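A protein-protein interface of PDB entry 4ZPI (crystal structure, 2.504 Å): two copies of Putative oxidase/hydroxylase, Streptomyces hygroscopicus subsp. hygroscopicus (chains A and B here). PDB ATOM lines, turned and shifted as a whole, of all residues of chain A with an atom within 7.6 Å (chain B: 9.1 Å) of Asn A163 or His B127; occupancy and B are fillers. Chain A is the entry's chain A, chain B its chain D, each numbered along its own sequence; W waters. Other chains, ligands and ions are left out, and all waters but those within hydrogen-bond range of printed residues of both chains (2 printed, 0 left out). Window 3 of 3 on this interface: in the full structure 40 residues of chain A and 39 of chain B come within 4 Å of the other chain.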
ATOM      1  N   ASN A 105       5.772   3.601   6.021  1.00  0.00           N
ATOM      2  CA  ASN A 105       5.221   2.296   5.738  1.00  0.00           C
ATOM      3  C   ASN A 105       4.851   1.450   6.986  1.00  0.00           C
ATOM      4  O   ASN A 105       3.900   0.666   6.953  1.00  0.00           O
ATOM      5  CB  ASN A 105       6.227   1.557   4.880  1.00  0.00           C
ATOM      6  CG  ASN A 105       5.626   0.390   4.161  1.00  0.00           C
ATOM      7  OD1 ASN A 105       4.598   0.523   3.491  1.00  0.00           O
ATOM      8  ND2 ASN A 105       6.245  -0.774   4.315  1.00  0.00           N
ATOM      9  N   SER A 106       5.584   1.621   8.084  1.00  0.00           N
ATOM     10  CA  SER A 106       5.419   0.751   9.250  1.00  0.00           C
ATOM     11  C   SER A 106       5.048   1.470  10.553  1.00  0.00           C
ATOM     12  O   SER A 106       5.227   0.917  11.637  1.00  0.00           O
ATOM     13  CB  SER A 106       6.702  -0.046   9.484  1.00  0.00           C
ATOM     14  OG  SER A 106       6.946  -0.932   8.412  1.00  0.00           O
ATOM     15  N   GLU A 107       4.535   2.689  10.453  1.00  0.00           N
ATOM     16  CA  GLU A 107       4.147   3.428  11.641  1.00  0.00           C
ATOM     17  C   GLU A 107       2.958   2.754  12.328  1.00  0.00           C
ATOM     18  O   GLU A 107       2.123   2.125  11.671  1.00  0.00           O
ATOM     19  CB  GLU A 107       3.837   4.879  11.284  1.00  0.00           C
ATOM     20  CG  GLU A 107       5.058   5.608  10.735  1.00  0.00           C
ATOM     21  CD  GLU A 107       6.291   5.448  11.637  1.00  0.00           C
ATOM     22  OE1 GLU A 107       6.175   5.612  12.875  1.00  0.00           O
ATOM     23  OE2 GLU A 107       7.379   5.149  11.110  1.00  0.00           O
ATOM     24  N   LEU A 108       2.901   2.884  13.655  1.00  0.00           N
ATOM     25  CA  LEU A 108       1.936   2.147  14.469  1.00  0.00           C
ATOM     26  C   LEU A 108       0.588   2.843  14.614  1.00  0.00           C
ATOM     27  O   LEU A 108       0.485   4.069  14.528  1.00  0.00           O
ATOM     28  CB  LEU A 108       2.513   1.891  15.855  1.00  0.00           C
ATOM     29  CG  LEU A 108       3.890   1.245  15.925  1.00  0.00           C
ATOM     30  CD1 LEU A 108       4.336   1.215  17.365  1.00  0.00           C
ATOM     31  CD2 LEU A 108       3.878  -0.161  15.314  1.00  0.00           C
ATOM     32  N   GLN A 115      -2.294  -3.282  18.685  1.00  0.00           N
ATOM     33  CA  GLN A 115      -1.522  -2.282  17.978  1.00  0.00           C
ATOM     34  C   GLN A 115      -1.028  -2.831  16.625  1.00  0.00           C
ATOM     35  O   GLN A 115      -0.353  -3.865  16.549  1.00  0.00           O
ATOM     36  CB  GLN A 115      -0.390  -1.811  18.877  1.00  0.00           C
ATOM     37  CG  GLN A 115       0.931  -1.534  18.223  1.00  0.00           C
ATOM     38  CD  GLN A 115       1.998  -1.277  19.270  1.00  0.00           C
ATOM     39  OE1 GLN A 115       1.804  -0.453  20.172  1.00  0.00           O
ATOM     40  NE2 GLN A 115       3.112  -2.006  19.184  1.00  0.00           N
ATOM     41  N   VAL A 116      -1.411  -2.148  15.550  1.00  0.00           N
ATOM     42  CA  VAL A 116      -1.094  -2.610  14.204  1.00  0.00           C
ATOM     43  C   VAL A 116      -0.035  -1.741  13.545  1.00  0.00           C
ATOM     44  O   VAL A 116       0.081  -0.551  13.836  1.00  0.00           O
ATOM     45  CB  VAL A 116      -2.363  -2.655  13.307  1.00  0.00           C
ATOM     46  CG1 VAL A 116      -3.365  -3.699  13.831  1.00  0.00           C
ATOM     47  CG2 VAL A 116      -3.009  -1.274  13.203  1.00  0.00           C
ATOM     48  N   GLY A 117       0.731  -2.340  12.639  1.00  0.00           N
ATOM     49  CA  GLY A 117       1.832  -1.653  11.993  1.00  0.00           C
ATOM     50  C   GLY A 117       1.765  -1.706  10.481  1.00  0.00           C
ATOM     51  O   GLY A 117       2.784  -1.553   9.800  1.00  0.00           O
ATOM     52  N   ARG A 118       0.570  -1.935   9.950  1.00  0.00           N
ATOM     53  CA  ARG A 118       0.353  -1.784   8.511  1.00  0.00           C
ATOM     54  C   ARG A 118      -0.890  -0.946   8.285  1.00  0.00           C
ATOM     55  O   ARG A 118      -1.888  -1.116   8.973  1.00  0.00           O
ATOM     56  CB  ARG A 118       0.216  -3.144   7.799  1.00  0.00           C
ATOM     57  CG  ARG A 118       1.532  -3.884   7.555  1.00  0.00           C
ATOM     58  CD  ARG A 118       2.330  -3.236   6.450  1.00  0.00           C
ATOM     59  NE  ARG A 118       3.656  -3.819   6.224  1.00  0.00           N
ATOM     60  CZ  ARG A 118       4.780  -3.364   6.781  1.00  0.00           C
ATOM     61  NH1 ARG A 118       4.738  -2.345   7.626  1.00  0.00           N
ATOM     62  NH2 ARG A 118       5.945  -3.928   6.502  1.00  0.00           N
ATOM     63  N   GLY A 158      13.901   5.817   1.796  1.00  0.00           N
ATOM     64  CA  GLY A 158      13.562   4.412   1.901  1.00  0.00           C
ATOM     65  C   GLY A 158      12.409   4.148   2.846  1.00  0.00           C
ATOM     66  O   GLY A 158      12.109   2.988   3.124  1.00  0.00           O
ATOM     67  N   SER A 159      11.753   5.204   3.324  1.00  0.00           N
ATOM     68  CA  SER A 159      10.764   5.055   4.387  1.00  0.00           C
ATOM     69  C   SER A 159       9.453   4.517   3.845  1.00  0.00           C
ATOM     70  O   SER A 159       8.587   4.088   4.620  1.00  0.00           O
ATOM     71  CB  SER A 159      10.527   6.386   5.120  1.00  0.00           C
ATOM     72  OG  SER A 159      10.068   7.410   4.238  1.00  0.00           O
ATOM     73  N   HIS A 160       9.308   4.531   2.518  1.00  0.00           N
ATOM     74  CA  HIS A 160       8.118   3.951   1.882  1.00  0.00           C
ATOM     75  C   HIS A 160       8.182   2.426   1.908  1.00  0.00           C
ATOM     76  O   HIS A 160       7.154   1.758   1.804  1.00  0.00           O
ATOM     77  CB  HIS A 160       7.942   4.458   0.447  1.00  0.00           C
ATOM     78  CG  HIS A 160       9.060   4.089  -0.479  1.00  0.00           C
ATOM     79  ND1 HIS A 160      10.386   4.335  -0.189  1.00  0.00           N
ATOM     80  CD2 HIS A 160       9.048   3.495  -1.694  1.00  0.00           C
ATOM     81  CE1 HIS A 160      11.142   3.903  -1.182  1.00  0.00           C
ATOM     82  NE2 HIS A 160      10.354   3.390  -2.107  1.00  0.00           N
ATOM     83  N   LYS A 161       9.379   1.865   2.060  1.00  0.00           N
ATOM     84  CA  LYS A 161       9.505   0.406   2.213  1.00  0.00           C
ATOM     85  C   LYS A 161      10.059   0.020   3.590  1.00  0.00           C
ATOM     86  O   LYS A 161      10.662  -1.040   3.744  1.00  0.00           O
ATOM     87  CB  LYS A 161      10.398  -0.183   1.113  1.00  0.00           C
ATOM     88  CG  LYS A 161       9.847  -0.019  -0.310  1.00  0.00           C
ATOM     89  CD  LYS A 161      10.871  -0.474  -1.347  1.00  0.00           C
ATOM     90  CE  LYS A 161      10.283  -0.459  -2.744  1.00  0.00           C
ATOM     91  NZ  LYS A 161      11.323  -0.775  -3.767  1.00  0.00           N
ATOM     92  N   ALA A 162       9.872   0.890   4.583  1.00  0.00           N
ATOM     93  CA  ALA A 162      10.370   0.639   5.937  1.00  0.00           C
ATOM     94  C   ALA A 162       9.697  -0.578   6.567  1.00  0.00           C
ATOM     95  O   ALA A 162       8.536  -0.860   6.294  1.00  0.00           O
ATOM     96  CB  ALA A 162      10.163   1.861   6.823  1.00  0.00           C
ATOM     97  N   ASN A 163      10.430  -1.286   7.418  1.00  0.00           N
ATOM     98  CA  ASN A 163       9.860  -2.405   8.159  1.00  0.00           C
ATOM     99  C   ASN A 163       9.729  -2.143   9.663  1.00  0.00           C
ATOM    100  O   ASN A 163       8.976  -2.826  10.359  1.00  0.00           O
ATOM    101  CB  ASN A 163      10.691  -3.659   7.914  1.00  0.00           C
ATOM    102  CG  ASN A 163      10.382  -4.298   6.575  1.00  0.00           C
ATOM    103  OD1 ASN A 163       9.217  -4.481   6.232  1.00  0.00           O
ATOM    104  ND2 ASN A 163      11.421  -4.632   5.810  1.00  0.00           N
ATOM    105  N   PHE A 164      10.463  -1.153  10.155  1.00  0.00           N
ATOM    106  CA  PHE A 164      10.402  -0.768  11.562  1.00  0.00           C
ATOM    107  C   PHE A 164       9.670   0.560  11.713  1.00  0.00           C
ATOM    108  O   PHE A 164       9.703   1.376  10.795  1.00  0.00           O
ATOM    109  CB  PHE A 164      11.803  -0.649  12.152  1.00  0.00           C
ATOM    110  CG  PHE A 164      12.594  -1.911  12.108  1.00  0.00           C
ATOM    111  CD1 PHE A 164      12.461  -2.861  13.098  1.00  0.00           C
ATOM    112  CD2 PHE A 164      13.495  -2.141  11.086  1.00  0.00           C
ATOM    113  CE1 PHE A 164      13.208  -4.029  13.068  1.00  0.00           C
ATOM    114  CE2 PHE A 164      14.240  -3.298  11.054  1.00  0.00           C
ATOM    115  CZ  PHE A 164      14.096  -4.246  12.052  1.00  0.00           C
ATOM    116  N   PRO A 165       8.998   0.784  12.861  1.00  0.00           N
ATOM    117  CA  PRO A 165       8.398   2.121  13.011  1.00  0.00           C
ATOM    118  C   PRO A 165       9.456   3.118  13.484  1.00  0.00           C
ATOM    119  O   PRO A 165      10.422   2.717  14.128  1.00  0.00           O
ATOM    120  CB  PRO A 165       7.288   1.906  14.047  1.00  0.00           C
ATOM    121  CG  PRO A 165       7.734   0.700  14.840  1.00  0.00           C
ATOM    122  CD  PRO A 165       8.647  -0.127  13.970  1.00  0.00           C
ATOM    123  N   LEU A 166       9.309   4.383  13.128  1.00  0.00           N
ATOM    124  CA  LEU A 166      10.280   5.395  13.522  1.00  0.00           C
ATOM    125  C   LEU A 166       9.756   6.286  14.653  1.00  0.00           C
ATOM    126  O   LEU A 166      10.451   6.507  15.635  1.00  0.00           O
ATOM    127  CB  LEU A 166      10.669   6.267  12.317  1.00  0.00           C
ATOM    128  CG  LEU A 166      11.858   7.228  12.468  1.00  0.00           C
ATOM    129  CD1 LEU A 166      13.120   6.454  12.817  1.00  0.00           C
ATOM    130  CD2 LEU A 166      12.068   8.071  11.196  1.00  0.00           C
ATOM    131  N   ASP B  13      -4.293 -18.666   7.491  1.00  0.00           N
ATOM    132  CA  ASP B  13      -3.157 -18.171   6.732  1.00  0.00           C
ATOM    133  C   ASP B  13      -2.760 -19.132   5.605  1.00  0.00           C
ATOM    134  O   ASP B  13      -2.568 -18.728   4.450  1.00  0.00           O
ATOM    135  CB  ASP B  13      -1.966 -17.948   7.670  1.00  0.00           C
ATOM    136  CG  ASP B  13      -0.691 -17.618   6.923  1.00  0.00           C
ATOM    137  OD1 ASP B  13      -0.706 -16.673   6.104  1.00  0.00           O
ATOM    138  OD2 ASP B  13       0.327 -18.310   7.148  1.00  0.00           O
ATOM    139  N   ASN B  80      -7.376  -6.749  10.889  1.00  0.00           N
ATOM    140  CA  ASN B  80      -6.491  -5.905  11.696  1.00  0.00           C
ATOM    141  C   ASN B  80      -6.388  -4.464  11.211  1.00  0.00           C
ATOM    142  O   ASN B  80      -5.307  -3.886  11.204  1.00  0.00           O
ATOM    143  CB  ASN B  80      -5.094  -6.524  11.766  1.00  0.00           C
ATOM    144  CG  ASN B  80      -5.015  -7.635  12.792  1.00  0.00           C
ATOM    145  OD1 ASN B  80      -5.126  -7.379  13.992  1.00  0.00           O
ATOM    146  ND2 ASN B  80      -4.853  -8.883  12.330  1.00  0.00           N
ATOM    147  N   HIS B 124      -3.403  -9.261   0.159  1.00  0.00           N
ATOM    148  CA  HIS B 124      -3.248  -9.332   1.607  1.00  0.00           C
ATOM    149  C   HIS B 124      -1.795  -9.511   2.011  1.00  0.00           C
ATOM    150  O   HIS B 124      -0.944  -9.788   1.185  1.00  0.00           O
ATOM    151  CB  HIS B 124      -4.094 -10.463   2.158  1.00  0.00           C
ATOM    152  CG  HIS B 124      -3.766 -11.787   1.556  1.00  0.00           C
ATOM    153  ND1 HIS B 124      -2.795 -12.620   2.073  1.00  0.00           N
ATOM    154  CD2 HIS B 124      -4.252 -12.408   0.452  1.00  0.00           C
ATOM    155  CE1 HIS B 124      -2.714 -13.709   1.327  1.00  0.00           C
ATOM    156  NE2 HIS B 124      -3.586 -13.605   0.337  1.00  0.00           N
ATOM    157  N   THR B 125      -1.502  -9.333   3.285  1.00  0.00           N
ATOM    158  CA  THR B 125      -0.121  -9.407   3.716  1.00  0.00           C
ATOM    159  C   THR B 125      -0.030  -9.831   5.177  1.00  0.00           C
ATOM    160  O   THR B 125      -1.033 -10.149   5.802  1.00  0.00           O
ATOM    161  CB  THR B 125       0.615  -8.055   3.499  1.00  0.00           C
ATOM    162  OG1 THR B 125       2.017  -8.250   3.715  1.00  0.00           O
ATOM    163  CG2 THR B 125       0.103  -6.987   4.439  1.00  0.00           C
ATOM    164  N   TYR B 126       1.187  -9.854   5.699  1.00  0.00           N
ATOM    165  CA  TYR B 126       1.445 -10.318   7.049  1.00  0.00           C
ATOM    166  C   TYR B 126       2.590  -9.517   7.631  1.00  0.00           C
ATOM    167  O   TYR B 126       3.596  -9.307   6.975  1.00  0.00           O
ATOM    168  CB  TYR B 126       1.780 -11.821   7.063  1.00  0.00           C
ATOM    169  CG  TYR B 126       2.379 -12.277   8.369  1.00  0.00           C
ATOM    170  CD1 TYR B 126       3.751 -12.234   8.582  1.00  0.00           C
ATOM    171  CD2 TYR B 126       1.566 -12.702   9.412  1.00  0.00           C
ATOM    172  CE1 TYR B 126       4.297 -12.617   9.792  1.00  0.00           C
ATOM    173  CE2 TYR B 126       2.107 -13.104  10.623  1.00  0.00           C
ATOM    174  CZ  TYR B 126       3.470 -13.055  10.802  1.00  0.00           C
ATOM    175  OH  TYR B 126       4.006 -13.442  12.002  1.00  0.00           O
ATOM    176  N   HIS B 127       2.452  -9.088   8.875  1.00  0.00           N
ATOM    177  CA  HIS B 127       3.468  -8.227   9.471  1.00  0.00           C
ATOM    178  C   HIS B 127       3.446  -8.333  10.989  1.00  0.00           C
ATOM    179  O   HIS B 127       2.389  -8.237  11.620  1.00  0.00           O
ATOM    180  CB  HIS B 127       3.257  -6.787   9.018  1.00  0.00           C
ATOM    181  CG  HIS B 127       4.298  -5.827   9.504  1.00  0.00           C
ATOM    182  ND1 HIS B 127       5.566  -5.770   8.965  1.00  0.00           N
ATOM    183  CD2 HIS B 127       4.247  -4.863  10.456  1.00  0.00           C
ATOM    184  CE1 HIS B 127       6.253  -4.815   9.571  1.00  0.00           C
ATOM    185  NE2 HIS B 127       5.476  -4.254  10.483  1.00  0.00           N
ATOM    186  N   ASP B 128       4.625  -8.579  11.548  1.00  0.00           N
ATOM    187  CA  ASP B 128       4.828  -8.673  12.986  1.00  0.00           C
ATOM    188  C   ASP B 128       3.706  -9.385  13.750  1.00  0.00           C
ATOM    189  O   ASP B 128       3.113  -8.819  14.659  1.00  0.00           O
ATOM    190  CB  ASP B 128       5.044  -7.269  13.550  1.00  0.00           C
ATOM    191  CG  ASP B 128       6.366  -6.653  13.078  1.00  0.00           C
ATOM    192  OD1 ASP B 128       7.189  -7.378  12.472  1.00  0.00           O
ATOM    193  OD2 ASP B 128       6.589  -5.452  13.329  1.00  0.00           O
ATOM    194  N   GLY B 129       3.421 -10.624  13.367  1.00  0.00           N
ATOM    195  CA  GLY B 129       2.477 -11.455  14.091  1.00  0.00           C
ATOM    196  C   GLY B 129       1.016 -11.337  13.708  1.00  0.00           C
ATOM    197  O   GLY B 129       0.187 -12.097  14.226  1.00  0.00           O
ATOM    198  N   LYS B 130       0.691 -10.394  12.814  1.00  0.00           N
ATOM    199  CA  LYS B 130      -0.695 -10.181  12.393  1.00  0.00           C
ATOM    200  C   LYS B 130      -0.906 -10.352  10.897  1.00  0.00           C
ATOM    201  O   LYS B 130      -0.044  -9.983  10.108  1.00  0.00           O
ATOM    202  CB  LYS B 130      -1.183  -8.787  12.805  1.00  0.00           C
ATOM    203  CG  LYS B 130      -1.362  -8.614  14.296  1.00  0.00           C
ATOM    204  CD  LYS B 130      -1.796  -7.198  14.647  1.00  0.00           C
ATOM    205  CE  LYS B 130      -1.847  -6.994  16.156  1.00  0.00           C
ATOM    206  NZ  LYS B 130      -0.497  -6.762  16.749  1.00  0.00           N
ATOM    207  N   LEU B 131      -2.064 -10.913  10.534  1.00  0.00           N
ATOM    208  CA  LEU B 131      -2.544 -10.958   9.148  1.00  0.00           C
ATOM    209  C   LEU B 131      -3.245  -9.668   8.785  1.00  0.00           C
ATOM    210  O   LEU B 131      -3.993  -9.126   9.598  1.00  0.00           O
ATOM    211  CB  LEU B 131      -3.522 -12.112   8.927  1.00  0.00           C
ATOM    212  CG  LEU B 131      -2.898 -13.495   9.050  1.00  0.00           C
ATOM    213  CD1 LEU B 131      -3.981 -14.575   9.149  1.00  0.00           C
ATOM    214  CD2 LEU B 131      -1.942 -13.748   7.894  1.00  0.00           C
ATOM    215  N   TYR B 132      -3.030  -9.193   7.558  1.00  0.00           N
ATOM    216  CA  TYR B 132      -3.732  -8.023   7.072  1.00  0.00           C
ATOM    217  C   TYR B 132      -4.480  -8.341   5.775  1.00  0.00           C
ATOM    218  O   TYR B 132      -3.935  -8.250   4.669  1.00  0.00           O
ATOM    219  CB  TYR B 132      -2.748  -6.859   6.892  1.00  0.00           C
ATOM    220  CG  TYR B 132      -2.148  -6.396   8.205  1.00  0.00           C
ATOM    221  CD1 TYR B 132      -2.780  -5.430   8.979  1.00  0.00           C
ATOM    222  CD2 TYR B 132      -0.960  -6.939   8.680  1.00  0.00           C
ATOM    223  CE1 TYR B 132      -2.240  -5.003  10.184  1.00  0.00           C
ATOM    224  CE2 TYR B 132      -0.418  -6.527   9.878  1.00  0.00           C
ATOM    225  CZ  TYR B 132      -1.065  -5.550  10.631  1.00  0.00           C
ATOM    226  OH  TYR B 132      -0.529  -5.130  11.838  1.00  0.00           O
ATOM    227  N   CYS B 133      -5.743  -8.708   5.923  1.00  0.00           N
ATOM    228  CA  CYS B 133      -6.564  -9.078   4.775  1.00  0.00           C
ATOM    229  C   CYS B 133      -7.657  -8.050   4.564  1.00  0.00           C
ATOM    230  O   CYS B 133      -8.549  -7.909   5.383  1.00  0.00           O
ATOM    231  CB  CYS B 133      -7.168 -10.468   4.964  1.00  0.00           C
ATOM    232  SG  CYS B 133      -5.933 -11.751   5.262  1.00  0.00           S
HETATM  233  O   HOH W   1       8.093  -3.386  12.834  1.00  0.00           O
HETATM  234  O   HOH W   2      -1.070  -5.653  19.566  1.00  0.00           O
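O of Gln A115 is in hydrogen-bond range of NZ of Lys B130 (2.9 Å). The backbone NH of Gly A117 sits at hydrogen-bond distance from the side-chain hydroxyl of Tyr B132. The guanidinium group (NH2) of Arg A118 is in hydrogen-bond range of a ring nitrogen (ND1) of His B127, 3.1 Å away.
NH1 of Arg A118 lies within hydrogen-bond range of O of Asn A105, 3.2 Å away. The guanidinium group (NH1) of Arg A118 sits at hydrogen-bond distance from the side-chain hydroxyl (OG) of Ser A106, 2.7 Å away. O of Asn A163 sits close to OG of Ser A106, 3.4 Å away. The side-chain amide oxygen of Asn A163 is in hydrogen-bond range of the guanidinium group of Arg A118 (3.3 Å). The side-chain amide nitrogen (ND2) of Asn B80 sits at hydrogen-bond distance from the backbone carbonyl oxygen (O) of Leu B131 (2.9 Å). The side-chain carboxylate (OD2) of Asp B128 lies within hydrogen-bond range of a ring nitrogen (NE2) of His B127 (3.3 Å).
O of Asn B80 touches CG1 of Val A116, 3.3 Å away. CG1 of Val A116 touches CD of Lys B130, 3.9 Å away. Tyr B132 touches Val A116 (OH to CB, 3.4 Å). CD2 of His B127 touches O of Gly A117 (3.7 Å). Tyr B132 touches Arg A118 (OH to N, 3.9 Å). His B127 touches Asn A163.
Of the printed residues of chain B, Gln A115 touches Lys B130. Gly A117 touches just these residues of chain B: His B127 (3.7 Å) and Tyr B132 (3.2 Å). Ser A159 touches none of the printed residues of chain B. Pro A165 touches none of the printed residues of chain B. Printed residues of chain A within 4 Å of Asn B80: Val A116. Of the printed residues of chain A, His B127 touches Gly A117 (3.7 Å), Arg A118 (3.1 Å) and Asn A163 (3.5 Å). Printed residues of chain A within 4 Å of Tyr B132: Val A116, Gly A117 and Arg A118. The nearest residue of chain B that does not touch Asn A163 is Asp B128 (4.6 Å). The nearest residue of chain A that does not touch His B127 is Ser A106 (4.1 Å). The nearest printed residue of chain A that does not touch Asn B80 is Arg A118 (4.9 Å).
Of the 12 printed residues of chain B, 4 touch a printed residue of chain A. Hydrophobic or aromatic side chains of chain B within 4 Å of the printed part of chain A: His B127 and Tyr B132.
No position is printed for both chains.
Water W1 bridges the side-chain carboxylate of Asp B128 and the backbone carbonyl oxygen of Asn A163. Water W2 lies within hydrogen-bond range of the backbone NH of Gln A115 (2.8 Å) and the side-chain amino group of Lys B130 (3.1 Å).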
